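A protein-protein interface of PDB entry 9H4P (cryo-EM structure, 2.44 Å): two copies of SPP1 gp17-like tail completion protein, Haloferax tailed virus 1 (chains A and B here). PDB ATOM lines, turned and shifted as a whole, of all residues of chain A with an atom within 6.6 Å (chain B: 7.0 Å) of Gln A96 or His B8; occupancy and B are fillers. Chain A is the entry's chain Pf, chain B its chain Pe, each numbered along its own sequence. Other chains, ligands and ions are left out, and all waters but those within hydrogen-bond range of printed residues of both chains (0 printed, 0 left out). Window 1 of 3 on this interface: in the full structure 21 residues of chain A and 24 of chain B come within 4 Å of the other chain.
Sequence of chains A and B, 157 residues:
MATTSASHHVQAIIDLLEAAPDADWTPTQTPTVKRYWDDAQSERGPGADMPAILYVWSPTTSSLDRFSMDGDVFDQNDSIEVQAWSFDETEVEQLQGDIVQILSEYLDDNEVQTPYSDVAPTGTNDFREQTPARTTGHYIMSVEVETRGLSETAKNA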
ATOM      1  N   ALA A  84     -21.185  11.090  -0.100  1.00  0.00           N
ATOM      2  CA  ALA A  84     -20.797   9.953   0.726  1.00  0.00           C
ATOM      3  C   ALA A  84     -21.980   8.993   0.887  1.00  0.00           C
ATOM      4  O   ALA A  84     -23.052   9.413   1.320  1.00  0.00           O
ATOM      5  CB  ALA A  84     -20.314  10.457   2.070  1.00  0.00           C
ATOM      6  N   GLU A  91     -21.592   7.138  10.141  1.00  0.00           N
ATOM      7  CA  GLU A  91     -20.409   7.066   9.294  1.00  0.00           C
ATOM      8  C   GLU A  91     -20.450   8.135   8.199  1.00  0.00           C
ATOM      9  O   GLU A  91     -19.425   8.767   7.949  1.00  0.00           O
ATOM     10  CB  GLU A  91     -20.215   5.664   8.715  1.00  0.00           C
ATOM     11  CG  GLU A  91     -18.876   5.468   8.031  1.00  0.00           C
ATOM     12  CD  GLU A  91     -18.647   4.047   7.563  1.00  0.00           C
ATOM     13  OE1 GLU A  91     -19.458   3.549   6.767  1.00  0.00           O
ATOM     14  OE2 GLU A  91     -17.663   3.437   8.009  1.00  0.00           O
ATOM     15  N   VAL A  92     -21.615   8.340   7.559  1.00  0.00           N
ATOM     16  CA  VAL A  92     -21.778   9.399   6.562  1.00  0.00           C
ATOM     17  C   VAL A  92     -21.540  10.779   7.179  1.00  0.00           C
ATOM     18  O   VAL A  92     -21.024  11.669   6.506  1.00  0.00           O
ATOM     19  CB  VAL A  92     -23.125   9.350   5.806  1.00  0.00           C
ATOM     20  CG1 VAL A  92     -23.161   8.234   4.773  1.00  0.00           C
ATOM     21  CG2 VAL A  92     -24.344   9.275   6.721  1.00  0.00           C
ATOM     22  N   GLU A  93     -21.934  10.949   8.446  1.00  0.00           N
ATOM     23  CA  GLU A  93     -21.770  12.203   9.166  1.00  0.00           C
ATOM     24  C   GLU A  93     -20.289  12.465   9.441  1.00  0.00           C
ATOM     25  O   GLU A  93     -19.830  13.596   9.290  1.00  0.00           O
ATOM     26  CB  GLU A  93     -22.625  12.155  10.432  1.00  0.00           C
ATOM     27  CG  GLU A  93     -22.674  13.451  11.208  1.00  0.00           C
ATOM     28  CD  GLU A  93     -23.389  13.255  12.527  1.00  0.00           C
ATOM     29  OE1 GLU A  93     -24.612  13.061  12.508  1.00  0.00           O
ATOM     30  OE2 GLU A  93     -22.716  13.274  13.565  1.00  0.00           O
ATOM     31  N   GLN A  94     -19.565  11.410   9.840  1.00  0.00           N
ATOM     32  CA  GLN A  94     -18.122  11.454  10.036  1.00  0.00           C
ATOM     33  C   GLN A  94     -17.415  11.733   8.708  1.00  0.00           C
ATOM     34  O   GLN A  94     -16.475  12.526   8.681  1.00  0.00           O
ATOM     35  CB  GLN A  94     -17.631  10.177  10.719  1.00  0.00           C
ATOM     36  CG  GLN A  94     -18.016  10.106  12.191  1.00  0.00           C
ATOM     37  CD  GLN A  94     -17.756   8.771  12.843  1.00  0.00           C
ATOM     38  OE1 GLN A  94     -17.430   7.782  12.192  1.00  0.00           O
ATOM     39  NE2 GLN A  94     -17.902   8.730  14.155  1.00  0.00           N
ATOM     40  N   LEU A  95     -17.887  11.102   7.617  1.00  0.00           N
ATOM     41  CA  LEU A  95     -17.321  11.294   6.286  1.00  0.00           C
ATOM     42  C   LEU A  95     -17.528  12.726   5.792  1.00  0.00           C
ATOM     43  O   LEU A  95     -16.625  13.277   5.168  1.00  0.00           O
ATOM     44  CB  LEU A  95     -17.897  10.266   5.306  1.00  0.00           C
ATOM     45  CG  LEU A  95     -16.974   9.101   4.931  1.00  0.00           C
ATOM     46  CD1 LEU A  95     -16.432   8.378   6.157  1.00  0.00           C
ATOM     47  CD2 LEU A  95     -17.694   8.115   4.024  1.00  0.00           C
ATOM     48  N   GLN A  96     -18.694  13.321   6.084  1.00  0.00           N
ATOM     49  CA  GLN A  96     -18.929  14.721   5.761  1.00  0.00           C
ATOM     50  C   GLN A  96     -17.908  15.619   6.462  1.00  0.00           C
ATOM     51  O   GLN A  96     -17.348  16.511   5.825  1.00  0.00           O
ATOM     52  CB  GLN A  96     -20.368  15.134   6.073  1.00  0.00           C
ATOM     53  CG  GLN A  96     -20.624  16.620   5.852  1.00  0.00           C
ATOM     54  CD  GLN A  96     -22.093  16.951   5.817  1.00  0.00           C
ATOM     55  OE1 GLN A  96     -22.681  17.349   6.822  1.00  0.00           O
ATOM     56  NE2 GLN A  96     -22.704  16.790   4.653  1.00  0.00           N
ATOM     57  N   GLY A  97     -17.694  15.387   7.769  1.00  0.00           N
ATOM     58  CA  GLY A  97     -16.666  16.063   8.546  1.00  0.00           C
ATOM     59  C   GLY A  97     -15.268  15.858   7.961  1.00  0.00           C
ATOM     60  O   GLY A  97     -14.521  16.822   7.822  1.00  0.00           O
ATOM     61  N   ASP A  98     -14.943  14.604   7.601  1.00  0.00           N
ATOM     62  CA  ASP A  98     -13.653  14.230   7.033  1.00  0.00           C
ATOM     63  C   ASP A  98     -13.394  14.928   5.693  1.00  0.00           C
ATOM     64  O   ASP A  98     -12.321  15.502   5.521  1.00  0.00           O
ATOM     65  CB  ASP A  98     -13.490  12.711   6.915  1.00  0.00           C
ATOM     66  CG  ASP A  98     -13.511  11.950   8.230  1.00  0.00           C
ATOM     67  OD1 ASP A  98     -13.295  12.572   9.287  1.00  0.00           O
ATOM     68  OD2 ASP A  98     -13.745  10.733   8.181  1.00  0.00           O
ATOM     69  N   ILE A  99     -14.362  14.878   4.758  1.00  0.00           N
ATOM     70  CA  ILE A  99     -14.228  15.484   3.433  1.00  0.00           C
ATOM     71  C   ILE A  99     -13.964  16.985   3.566  1.00  0.00           C
ATOM     72  O   ILE A  99     -13.070  17.507   2.900  1.00  0.00           O
ATOM     73  CB  ILE A  99     -15.442  15.187   2.519  1.00  0.00           C
ATOM     74  CG1 ILE A  99     -15.588  13.691   2.219  1.00  0.00           C
ATOM     75  CG2 ILE A  99     -15.366  15.995   1.226  1.00  0.00           C
ATOM     76  CD1 ILE A  99     -16.997  13.256   1.855  1.00  0.00           C
ATOM     77  N   VAL A 100     -14.743  17.661   4.426  1.00  0.00           N
ATOM     78  CA  VAL A 100     -14.550  19.076   4.720  1.00  0.00           C
ATOM     79  C   VAL A 100     -13.136  19.313   5.256  1.00  0.00           C
ATOM     80  O   VAL A 100     -12.460  20.222   4.777  1.00  0.00           O
ATOM     81  CB  VAL A 100     -15.646  19.653   5.647  1.00  0.00           C
ATOM     82  CG1 VAL A 100     -15.307  21.043   6.179  1.00  0.00           C
ATOM     83  CG2 VAL A 100     -17.009  19.676   4.967  1.00  0.00           C
ATOM     84  N   GLN A 101     -12.696  18.490   6.221  1.00  0.00           N
ATOM     85  CA  GLN A 101     -11.363  18.610   6.798  1.00  0.00           C
ATOM     86  C   GLN A 101     -10.272  18.432   5.736  1.00  0.00           C
ATOM     87  O   GLN A 101      -9.396  19.289   5.624  1.00  0.00           O
ATOM     88  CB  GLN A 101     -11.189  17.680   8.004  1.00  0.00           C
ATOM     89  CG  GLN A 101     -11.872  18.177   9.273  1.00  0.00           C
ATOM     90  CD  GLN A 101     -11.212  19.388   9.889  1.00  0.00           C
ATOM     91  OE1 GLN A 101     -11.494  20.531   9.537  1.00  0.00           O
ATOM     92  NE2 GLN A 101     -10.320  19.140  10.832  1.00  0.00           N
ATOM     93  N   GLY A 123     -20.399  24.534   0.791  1.00  0.00           N
ATOM     94  CA  GLY A 123     -21.626  24.147   1.466  1.00  0.00           C
ATOM     95  C   GLY A 123     -21.695  22.635   1.647  1.00  0.00           C
ATOM     96  O   GLY A 123     -20.880  21.908   1.078  1.00  0.00           O
ATOM     97  N   THR A 124     -22.671  22.175   2.442  1.00  0.00           N
ATOM     98  CA  THR A 124     -22.851  20.756   2.714  1.00  0.00           C
ATOM     99  C   THR A 124     -24.341  20.424   2.795  1.00  0.00           C
ATOM    100  O   THR A 124     -25.147  21.274   3.171  1.00  0.00           O
ATOM    101  CB  THR A 124     -22.130  20.313   3.998  1.00  0.00           C
ATOM    102  OG1 THR A 124     -22.707  20.981   5.121  1.00  0.00           O
ATOM    103  CG2 THR A 124     -20.633  20.544   3.990  1.00  0.00           C
ATOM    104  N   ASN A 125     -24.681  19.172   2.463  1.00  0.00           N
ATOM    105  CA  ASN A 125     -26.058  18.705   2.462  1.00  0.00           C
ATOM    106  C   ASN A 125     -26.179  17.427   3.288  1.00  0.00           C
ATOM    107  O   ASN A 125     -25.278  16.590   3.295  1.00  0.00           O
ATOM    108  CB  ASN A 125     -26.573  18.455   1.041  1.00  0.00           C
ATOM    109  CG  ASN A 125     -26.416  19.646   0.122  1.00  0.00           C
ATOM    110  OD1 ASN A 125     -27.099  20.654   0.280  1.00  0.00           O
ATOM    111  ND2 ASN A 125     -25.527  19.538  -0.851  1.00  0.00           N
ATOM    112  N   ASP A 126     -27.318  17.306   3.976  1.00  0.00           N
ATOM    113  CA  ASP A 126     -27.747  16.079   4.621  1.00  0.00           C
ATOM    114  C   ASP A 126     -28.972  15.561   3.868  1.00  0.00           C
ATOM    115  O   ASP A 126     -29.880  16.339   3.576  1.00  0.00           O
ATOM    116  CB  ASP A 126     -28.034  16.357   6.100  1.00  0.00           C
ATOM    117  CG  ASP A 126     -28.342  15.134   6.947  1.00  0.00           C
ATOM    118  OD1 ASP A 126     -28.392  14.018   6.396  1.00  0.00           O
ATOM    119  OD2 ASP A 126     -28.533  15.314   8.164  1.00  0.00           O
ATOM    120  N   ARG A 128     -30.222  12.264   4.899  1.00  0.00           N
ATOM    121  CA  ARG A 128     -30.578  11.103   5.711  1.00  0.00           C
ATOM    122  C   ARG A 128     -32.091  10.986   5.909  1.00  0.00           C
ATOM    123  O   ARG A 128     -32.590   9.875   6.091  1.00  0.00           O
ATOM    124  CB  ARG A 128     -29.845  11.122   7.054  1.00  0.00           C
ATOM    125  CG  ARG A 128     -28.360  10.810   6.934  1.00  0.00           C
ATOM    126  CD  ARG A 128     -27.592  10.946   8.237  1.00  0.00           C
ATOM    127  NE  ARG A 128     -27.601  12.322   8.726  1.00  0.00           N
ATOM    128  CZ  ARG A 128     -27.003  12.760   9.833  1.00  0.00           C
ATOM    129  NH1 ARG A 128     -27.094  14.036  10.164  1.00  0.00           N
ATOM    130  NH2 ARG A 128     -26.314  11.932  10.601  1.00  0.00           N
ATOM    131  N   MET A 141     -24.990  11.807   2.411  1.00  0.00           N
ATOM    132  CA  MET A 141     -24.669  13.192   2.731  1.00  0.00           C
ATOM    133  C   MET A 141     -23.658  13.697   1.699  1.00  0.00           C
ATOM    134  O   MET A 141     -23.007  12.886   1.040  1.00  0.00           O
ATOM    135  CB  MET A 141     -24.090  13.304   4.150  1.00  0.00           C
ATOM    136  CG  MET A 141     -25.049  12.832   5.244  1.00  0.00           C
ATOM    137  SD  MET A 141     -24.428  12.960   6.939  1.00  0.00           S
ATOM    138  CE  MET A 141     -24.680  14.703   7.265  1.00  0.00           C
ATOM    139  N   SER A 142     -23.528  15.026   1.542  1.00  0.00           N
ATOM    140  CA  SER A 142     -22.641  15.555   0.513  1.00  0.00           C
ATOM    141  C   SER A 142     -21.925  16.843   0.929  1.00  0.00           C
ATOM    142  O   SER A 142     -22.376  17.566   1.816  1.00  0.00           O
ATOM    143  CB  SER A 142     -23.350  15.703  -0.815  1.00  0.00           C
ATOM    144  OG  SER A 142     -24.171  16.861  -0.835  1.00  0.00           O
ATOM    145  N   VAL A 143     -20.795  17.093   0.250  1.00  0.00           N
ATOM    146  CA  VAL A 143     -20.028  18.328   0.340  1.00  0.00           C
ATOM    147  C   VAL A 143     -20.015  18.970  -1.047  1.00  0.00           C
ATOM    148  O   VAL A 143     -19.710  18.310  -2.041  1.00  0.00           O
ATOM    149  CB  VAL A 143     -18.596  18.076   0.869  1.00  0.00           C
ATOM    150  CG1 VAL A 143     -17.758  19.347   0.942  1.00  0.00           C
ATOM    151  CG2 VAL A 143     -18.598  17.383   2.223  1.00  0.00           C
ATOM    152  N   SER B   5     -22.270  19.183  22.893  1.00  0.00           N
ATOM    153  CA  SER B   5     -20.957  18.867  22.331  1.00  0.00           C
ATOM    154  C   SER B   5     -21.054  17.957  21.096  1.00  0.00           C
ATOM    155  O   SER B   5     -20.112  17.221  20.807  1.00  0.00           O
ATOM    156  CB  SER B   5     -20.012  18.321  23.391  1.00  0.00           C
ATOM    157  OG  SER B   5     -18.687  18.217  22.894  1.00  0.00           O
ATOM    158  N   ALA B   6     -22.166  18.047  20.344  1.00  0.00           N
ATOM    159  CA  ALA B   6     -22.509  17.118  19.270  1.00  0.00           C
ATOM    160  C   ALA B   6     -21.666  17.342  18.011  1.00  0.00           C
ATOM    161  O   ALA B   6     -21.162  18.439  17.774  1.00  0.00           O
ATOM    162  CB  ALA B   6     -23.985  17.205  18.971  1.00  0.00           C
ATOM    163  N   SER B   7     -21.572  16.279  17.196  1.00  0.00           N
ATOM    164  CA  SER B   7     -20.819  16.207  15.949  1.00  0.00           C
ATOM    165  C   SER B   7     -21.453  17.048  14.833  1.00  0.00           C
ATOM    166  O   SER B   7     -20.729  17.643  14.033  1.00  0.00           O
ATOM    167  CB  SER B   7     -20.635  14.756  15.559  1.00  0.00           C
ATOM    168  OG  SER B   7     -20.420  14.602  14.166  1.00  0.00           O
ATOM    169  N   HIS B   8     -22.796  17.103  14.791  1.00  0.00           N
ATOM    170  CA  HIS B   8     -23.556  17.656  13.672  1.00  0.00           C
ATOM    171  C   HIS B   8     -24.820  18.347  14.186  1.00  0.00           C
ATOM    172  O   HIS B   8     -25.318  17.985  15.249  1.00  0.00           O
ATOM    173  CB  HIS B   8     -23.916  16.512  12.716  1.00  0.00           C
ATOM    174  CG  HIS B   8     -24.558  16.913  11.431  1.00  0.00           C
ATOM    175  ND1 HIS B   8     -25.930  17.019  11.275  1.00  0.00           N
ATOM    176  CD2 HIS B   8     -24.018  17.186  10.226  1.00  0.00           C
ATOM    177  CE1 HIS B   8     -26.201  17.363  10.031  1.00  0.00           C
ATOM    178  NE2 HIS B   8     -25.042  17.473   9.368  1.00  0.00           N
ATOM    179  N   HIS B   9     -25.351  19.304  13.411  1.00  0.00           N
ATOM    180  CA  HIS B   9     -26.427  20.181  13.858  1.00  0.00           C
ATOM    181  C   HIS B   9     -27.720  19.439  14.217  1.00  0.00           C
ATOM    182  O   HIS B   9     -28.383  19.836  15.174  1.00  0.00           O
ATOM    183  CB  HIS B   9     -26.618  21.379  12.911  1.00  0.00           C
ATOM    184  CG  HIS B   9     -26.654  21.070  11.447  1.00  0.00           C
ATOM    185  ND1 HIS B   9     -25.508  20.881  10.690  1.00  0.00           N
ATOM    186  CD2 HIS B   9     -27.688  21.007  10.578  1.00  0.00           C
ATOM    187  CE1 HIS B   9     -25.841  20.678   9.429  1.00  0.00           C
ATOM    188  NE2 HIS B   9     -27.173  20.749   9.335  1.00  0.00           N
ATOM    189  N   VAL B  10     -28.077  18.382  13.467  1.00  0.00           N
ATOM    190  CA  VAL B  10     -29.309  17.642  13.721  1.00  0.00           C
ATOM    191  C   VAL B  10     -29.268  17.014  15.115  1.00  0.00           C
ATOM    192  O   VAL B  10     -30.234  17.140  15.869  1.00  0.00           O
ATOM    193  CB  VAL B  10     -29.632  16.609  12.618  1.00  0.00           C
ATOM    194  CG1 VAL B  10     -30.778  15.678  12.995  1.00  0.00           C
ATOM    195  CG2 VAL B  10     -29.919  17.279  11.282  1.00  0.00           C
ATOM    196  N   GLN B  11     -28.151  16.349  15.445  1.00  0.00           N
ATOM    197  CA  GLN B  11     -27.996  15.737  16.756  1.00  0.00           C
ATOM    198  C   GLN B  11     -27.875  16.813  17.834  1.00  0.00           C
ATOM    199  O   GLN B  11     -28.338  16.600  18.953  1.00  0.00           O
ATOM    200  CB  GLN B  11     -26.823  14.753  16.790  1.00  0.00           C
ATOM    201  CG  GLN B  11     -26.750  13.927  18.072  1.00  0.00           C
ATOM    202  CD  GLN B  11     -27.956  13.043  18.284  1.00  0.00           C
ATOM    203  OE1 GLN B  11     -28.351  12.277  17.409  1.00  0.00           O
ATOM    204  NE2 GLN B  11     -28.548  13.133  19.462  1.00  0.00           N
ATOM    205  N   ALA B  12     -27.261  17.959  17.498  1.00  0.00           N
ATOM    206  CA  ALA B  12     -27.099  19.065  18.434  1.00  0.00           C
ATOM    207  C   ALA B  12     -28.452  19.597  18.910  1.00  0.00           C
ATOM    208  O   ALA B  12     -28.622  19.834  20.107  1.00  0.00           O
ATOM    209  CB  ALA B  12     -26.230  20.149  17.837  1.00  0.00           C
ATOM    210  N   ILE B  13     -29.407  19.762  17.981  1.00  0.00           N
ATOM    211  CA  ILE B  13     -30.730  20.275  18.316  1.00  0.00           C
ATOM    212  C   ILE B  13     -31.570  19.206  19.020  1.00  0.00           C
ATOM    213  O   ILE B  13     -32.323  19.541  19.936  1.00  0.00           O
ATOM    214  CB  ILE B  13     -31.407  20.962  17.107  1.00  0.00           C
ATOM    215  CG1 ILE B  13     -30.663  22.265  16.790  1.00  0.00           C
ATOM    216  CG2 ILE B  13     -32.900  21.182  17.336  1.00  0.00           C
ATOM    217  CD1 ILE B  13     -31.436  23.307  16.015  1.00  0.00           C
ATOM    218  N   ILE B  14     -31.408  17.932  18.633  1.00  0.00           N
ATOM    219  CA  ILE B  14     -32.041  16.833  19.352  1.00  0.00           C
ATOM    220  C   ILE B  14     -31.580  16.817  20.811  1.00  0.00           C
ATOM    221  O   ILE B  14     -32.418  16.698  21.705  1.00  0.00           O
ATOM    222  CB  ILE B  14     -31.858  15.482  18.627  1.00  0.00           C
ATOM    223  CG1 ILE B  14     -32.667  15.466  17.327  1.00  0.00           C
ATOM    224  CG2 ILE B  14     -32.234  14.307  19.526  1.00  0.00           C
ATOM    225  CD1 ILE B  14     -32.354  14.325  16.392  1.00  0.00           C
ATOM    226  N   ASP B  15     -30.263  16.958  21.040  1.00  0.00           N
ATOM    227  CA  ASP B  15     -29.687  17.023  22.377  1.00  0.00           C
ATOM    228  C   ASP B  15     -30.262  18.195  23.182  1.00  0.00           C
ATOM    229  O   ASP B  15     -30.484  18.037  24.380  1.00  0.00           O
ATOM    230  CB  ASP B  15     -28.156  17.070  22.340  1.00  0.00           C
ATOM    231  CG  ASP B  15     -27.450  15.795  21.907  1.00  0.00           C
ATOM    232  OD1 ASP B  15     -28.133  14.786  21.658  1.00  0.00           O
ATOM    233  OD2 ASP B  15     -26.210  15.827  21.826  1.00  0.00           O
ATOM    234  N   TRP B  37     -35.827  10.393  10.114  1.00  0.00           N
ATOM    235  CA  TRP B  37     -35.614   9.081   9.514  1.00  0.00           C
ATOM    236  C   TRP B  37     -35.661   7.933  10.533  1.00  0.00           C
ATOM    237  O   TRP B  37     -35.418   6.787  10.151  1.00  0.00           O
ATOM    238  CB  TRP B  37     -34.315   9.078   8.687  1.00  0.00           C
ATOM    239  CG  TRP B  37     -33.051   9.288   9.469  1.00  0.00           C
ATOM    240  CD1 TRP B  37     -32.303   8.310  10.056  1.00  0.00           C
ATOM    241  CD2 TRP B  37     -32.363  10.533   9.741  1.00  0.00           C
ATOM    242  NE1 TRP B  37     -31.213   8.855  10.677  1.00  0.00           N
ATOM    243  CE2 TRP B  37     -31.215  10.215  10.503  1.00  0.00           C
ATOM    244  CE3 TRP B  37     -32.592  11.887   9.433  1.00  0.00           C
ATOM    245  CZ2 TRP B  37     -30.315  11.190  10.951  1.00  0.00           C
ATOM    246  CZ3 TRP B  37     -31.705  12.849   9.875  1.00  0.00           C
ATOM    247  CH2 TRP B  37     -30.579  12.504  10.628  1.00  0.00           C
ATOM    248  N   SER B  58     -32.243  18.391   8.826  1.00  0.00           N
ATOM    249  CA  SER B  58     -31.701  19.548   8.127  1.00  0.00           C
ATOM    250  C   SER B  58     -32.292  19.622   6.715  1.00  0.00           C
ATOM    251  O   SER B  58     -31.914  18.825   5.855  1.00  0.00           O
ATOM    252  CB  SER B  58     -30.189  19.499   8.111  1.00  0.00           C
ATOM    253  OG  SER B  58     -29.645  20.675   7.529  1.00  0.00           O
ATOM    254  N   SER B  62     -26.284  23.696   4.256  1.00  0.00           N
ATOM    255  CA  SER B  62     -25.458  24.508   5.145  1.00  0.00           C
ATOM    256  C   SER B  62     -24.394  25.253   4.334  1.00  0.00           C
ATOM    257  O   SER B  62     -23.758  24.645   3.479  1.00  0.00           O
ATOM    258  CB  SER B  62     -24.789  23.641   6.188  1.00  0.00           C
ATOM    259  OG  SER B  62     -25.719  23.169   7.151  1.00  0.00           O
ATOM    260  N   GLN B  76     -19.659  29.085   9.401  1.00  0.00           N
ATOM    261  CA  GLN B  76     -20.614  28.041   9.051  1.00  0.00           C
ATOM    262  C   GLN B  76     -22.026  28.466   9.459  1.00  0.00           C
ATOM    263  O   GLN B  76     -22.246  28.867  10.604  1.00  0.00           O
ATOM    264  CB  GLN B  76     -20.215  26.710   9.697  1.00  0.00           C
ATOM    265  CG  GLN B  76     -21.234  25.593   9.487  1.00  0.00           C
ATOM    266  CD  GLN B  76     -20.730  24.202   9.784  1.00  0.00           C
ATOM    267  OE1 GLN B  76     -19.549  23.981  10.038  1.00  0.00           O
ATOM    268  NE2 GLN B  76     -21.635  23.238   9.742  1.00  0.00           N
ATOM    269  N   ASP B  78     -26.018  26.888   9.401  1.00  0.00           N
ATOM    270  CA  ASP B  78     -26.730  25.613   9.380  1.00  0.00           C
ATOM    271  C   ASP B  78     -28.242  25.836   9.497  1.00  0.00           C
ATOM    272  O   ASP B  78     -28.675  26.811  10.106  1.00  0.00           O
ATOM    273  CB  ASP B  78     -26.229  24.687  10.496  1.00  0.00           C
ATOM    274  CG  ASP B  78     -24.756  24.317  10.405  1.00  0.00           C
ATOM    275  OD1 ASP B  78     -24.297  23.977   9.303  1.00  0.00           O
ATOM    276  OD2 ASP B  78     -24.082  24.358  11.448  1.00  0.00           O
ATOM    277  N   ILE B  80     -32.234  23.867  10.078  1.00  0.00           N
ATOM    278  CA  ILE B  80     -32.977  22.753  10.664  1.00  0.00           C
ATOM    279  C   ILE B  80     -34.477  23.045  10.609  1.00  0.00           C
ATOM    280  O   ILE B  80     -34.885  24.205  10.629  1.00  0.00           O
ATOM    281  CB  ILE B  80     -32.467  22.419  12.088  1.00  0.00           C
ATOM    282  CG1 ILE B  80     -31.184  21.587  11.980  1.00  0.00           C
ATOM    283  CG2 ILE B  80     -33.511  21.706  12.948  1.00  0.00           C
ATOM    284  CD1 ILE B  80     -30.444  21.362  13.274  1.00  0.00           C
ATOM    285  N   PRO B 115     -21.890  23.642  20.517  1.00  0.00           N
ATOM    286  CA  PRO B 115     -20.719  24.024  19.717  1.00  0.00           C
ATOM    287  C   PRO B 115     -20.877  25.235  18.782  1.00  0.00           C
ATOM    288  O   PRO B 115     -20.030  25.441  17.914  1.00  0.00           O
ATOM    289  CB  PRO B 115     -20.429  22.730  18.927  1.00  0.00           C
ATOM    290  CG  PRO B 115     -21.793  22.119  18.694  1.00  0.00           C
ATOM    291  CD  PRO B 115     -22.575  22.462  19.947  1.00  0.00           C
ATOM    292  N   TYR B 116     -21.931  26.055  18.979  1.00  0.00           N
ATOM    293  CA  TYR B 116     -22.278  27.170  18.095  1.00  0.00           C
ATOM    294  C   TYR B 116     -22.073  28.516  18.793  1.00  0.00           C
ATOM    295  O   TYR B 116     -21.834  28.547  19.996  1.00  0.00           O
ATOM    296  CB  TYR B 116     -23.704  27.000  17.555  1.00  0.00           C
ATOM    297  CG  TYR B 116     -23.847  25.682  16.847  1.00  0.00           C
ATOM    298  CD1 TYR B 116     -23.126  25.447  15.685  1.00  0.00           C
ATOM    299  CD2 TYR B 116     -24.601  24.644  17.380  1.00  0.00           C
ATOM    300  CE1 TYR B 116     -23.187  24.226  15.039  1.00  0.00           C
ATOM    301  CE2 TYR B 116     -24.681  23.415  16.741  1.00  0.00           C
ATOM    302  CZ  TYR B 116     -23.968  23.212  15.569  1.00  0.00           C
ATOM    303  OH  TYR B 116     -24.027  22.015  14.923  1.00  0.00           O
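Of the 19 printed residues of chain B, 6 touch a printed residue of chain A. Printed residues of chain B that touch a printed residue of chain A: Ser B7, His B8, Val B10, Trp B37, Ser B58 and Ser B62. Of the 20 printed residues of chain A, 7 touch a printed residue of chain B. Hydrophobic or aromatic side chains of chain A that line the printed part of chain B: Met A141. Among the printed residues, 11 pairs touch across the chains.
No position is printed for both chains.
Among the printed residues, merely in contact across the chains: Gly A123 with Ser B62 (3.0 Å), Arg A128 with Trp B37 (3.2 Å), Glu A93 with His B8 (3.3 Å), Met A141 with His B8 (3.5 Å), Asp A126 with His B8 (3.6 Å), Asp A126 with Val B10 (3.9 Å) and Asp A126 with Ser B58 (3.9 Å).
Of the printed residues of chain B, Glu A93 touches Ser B7 and His B8. Of chain B, only His B8 (3.5 Å) comes within 4 Å of Gln A96. Printed residues of chain A within 4 Å of Trp B37: Arg A128 (3.2 Å). Printed residues of chain A within 4 Å of Ser B58: Asp A126 (3.9 Å). The nearest residue of chain B that does not touch Gln A96 is His B9 (5.3 Å). The nearest residue of chain A that does not touch His B8 is Thr A124 (6.0 Å). The nearest printed residue of chain A that does not touch Trp B37 is Asp A126 (4.3 Å).
The guanidinium group (NH1) of Arg A128 is in salt-bridge range of the side-chain carboxylate (OD2) of Asp A126, at 2.8 Å. The side-chain amide nitrogen (NE2) of Gln A96 is in hydrogen-bond range of the backbone carbonyl oxygen (O) of Ser A142 (3.0 Å). N of Ala A84 lies within hydrogen-bond range of O of Met A141, at 2.8 Å. The side-chain amide nitrogen (NE2) of Gln A96 lies within hydrogen-bond range of the backbone carbonyl oxygen (O) of Asn A125, at 2.9 Å. The guanidinium group (NH2) of Arg A128 is in salt-bridge range of the side-chain carboxylate (OE1) of Glu A93 (2.8 Å). The guanidinium group (NE) of Arg A128 is in hydrogen-bond range of the side-chain sulfur (SD) of Met A141 (3.7 Å).
OE1 of Gln A96 is in hydrogen-bond range of NE2 of His B8 (3.5 Å). ND1 of His B8 is in hydrogen-bond range of NH1 of Arg A128, at 3.4 Å. OG of Ser B7 is in hydrogen-bond range of OE2 of Glu A93 (2.7 Å). The backbone NH (N) of Ser B62 sits at hydrogen-bond distance from the backbone carbonyl oxygen (O) of Thr A124 (2.9 Å).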
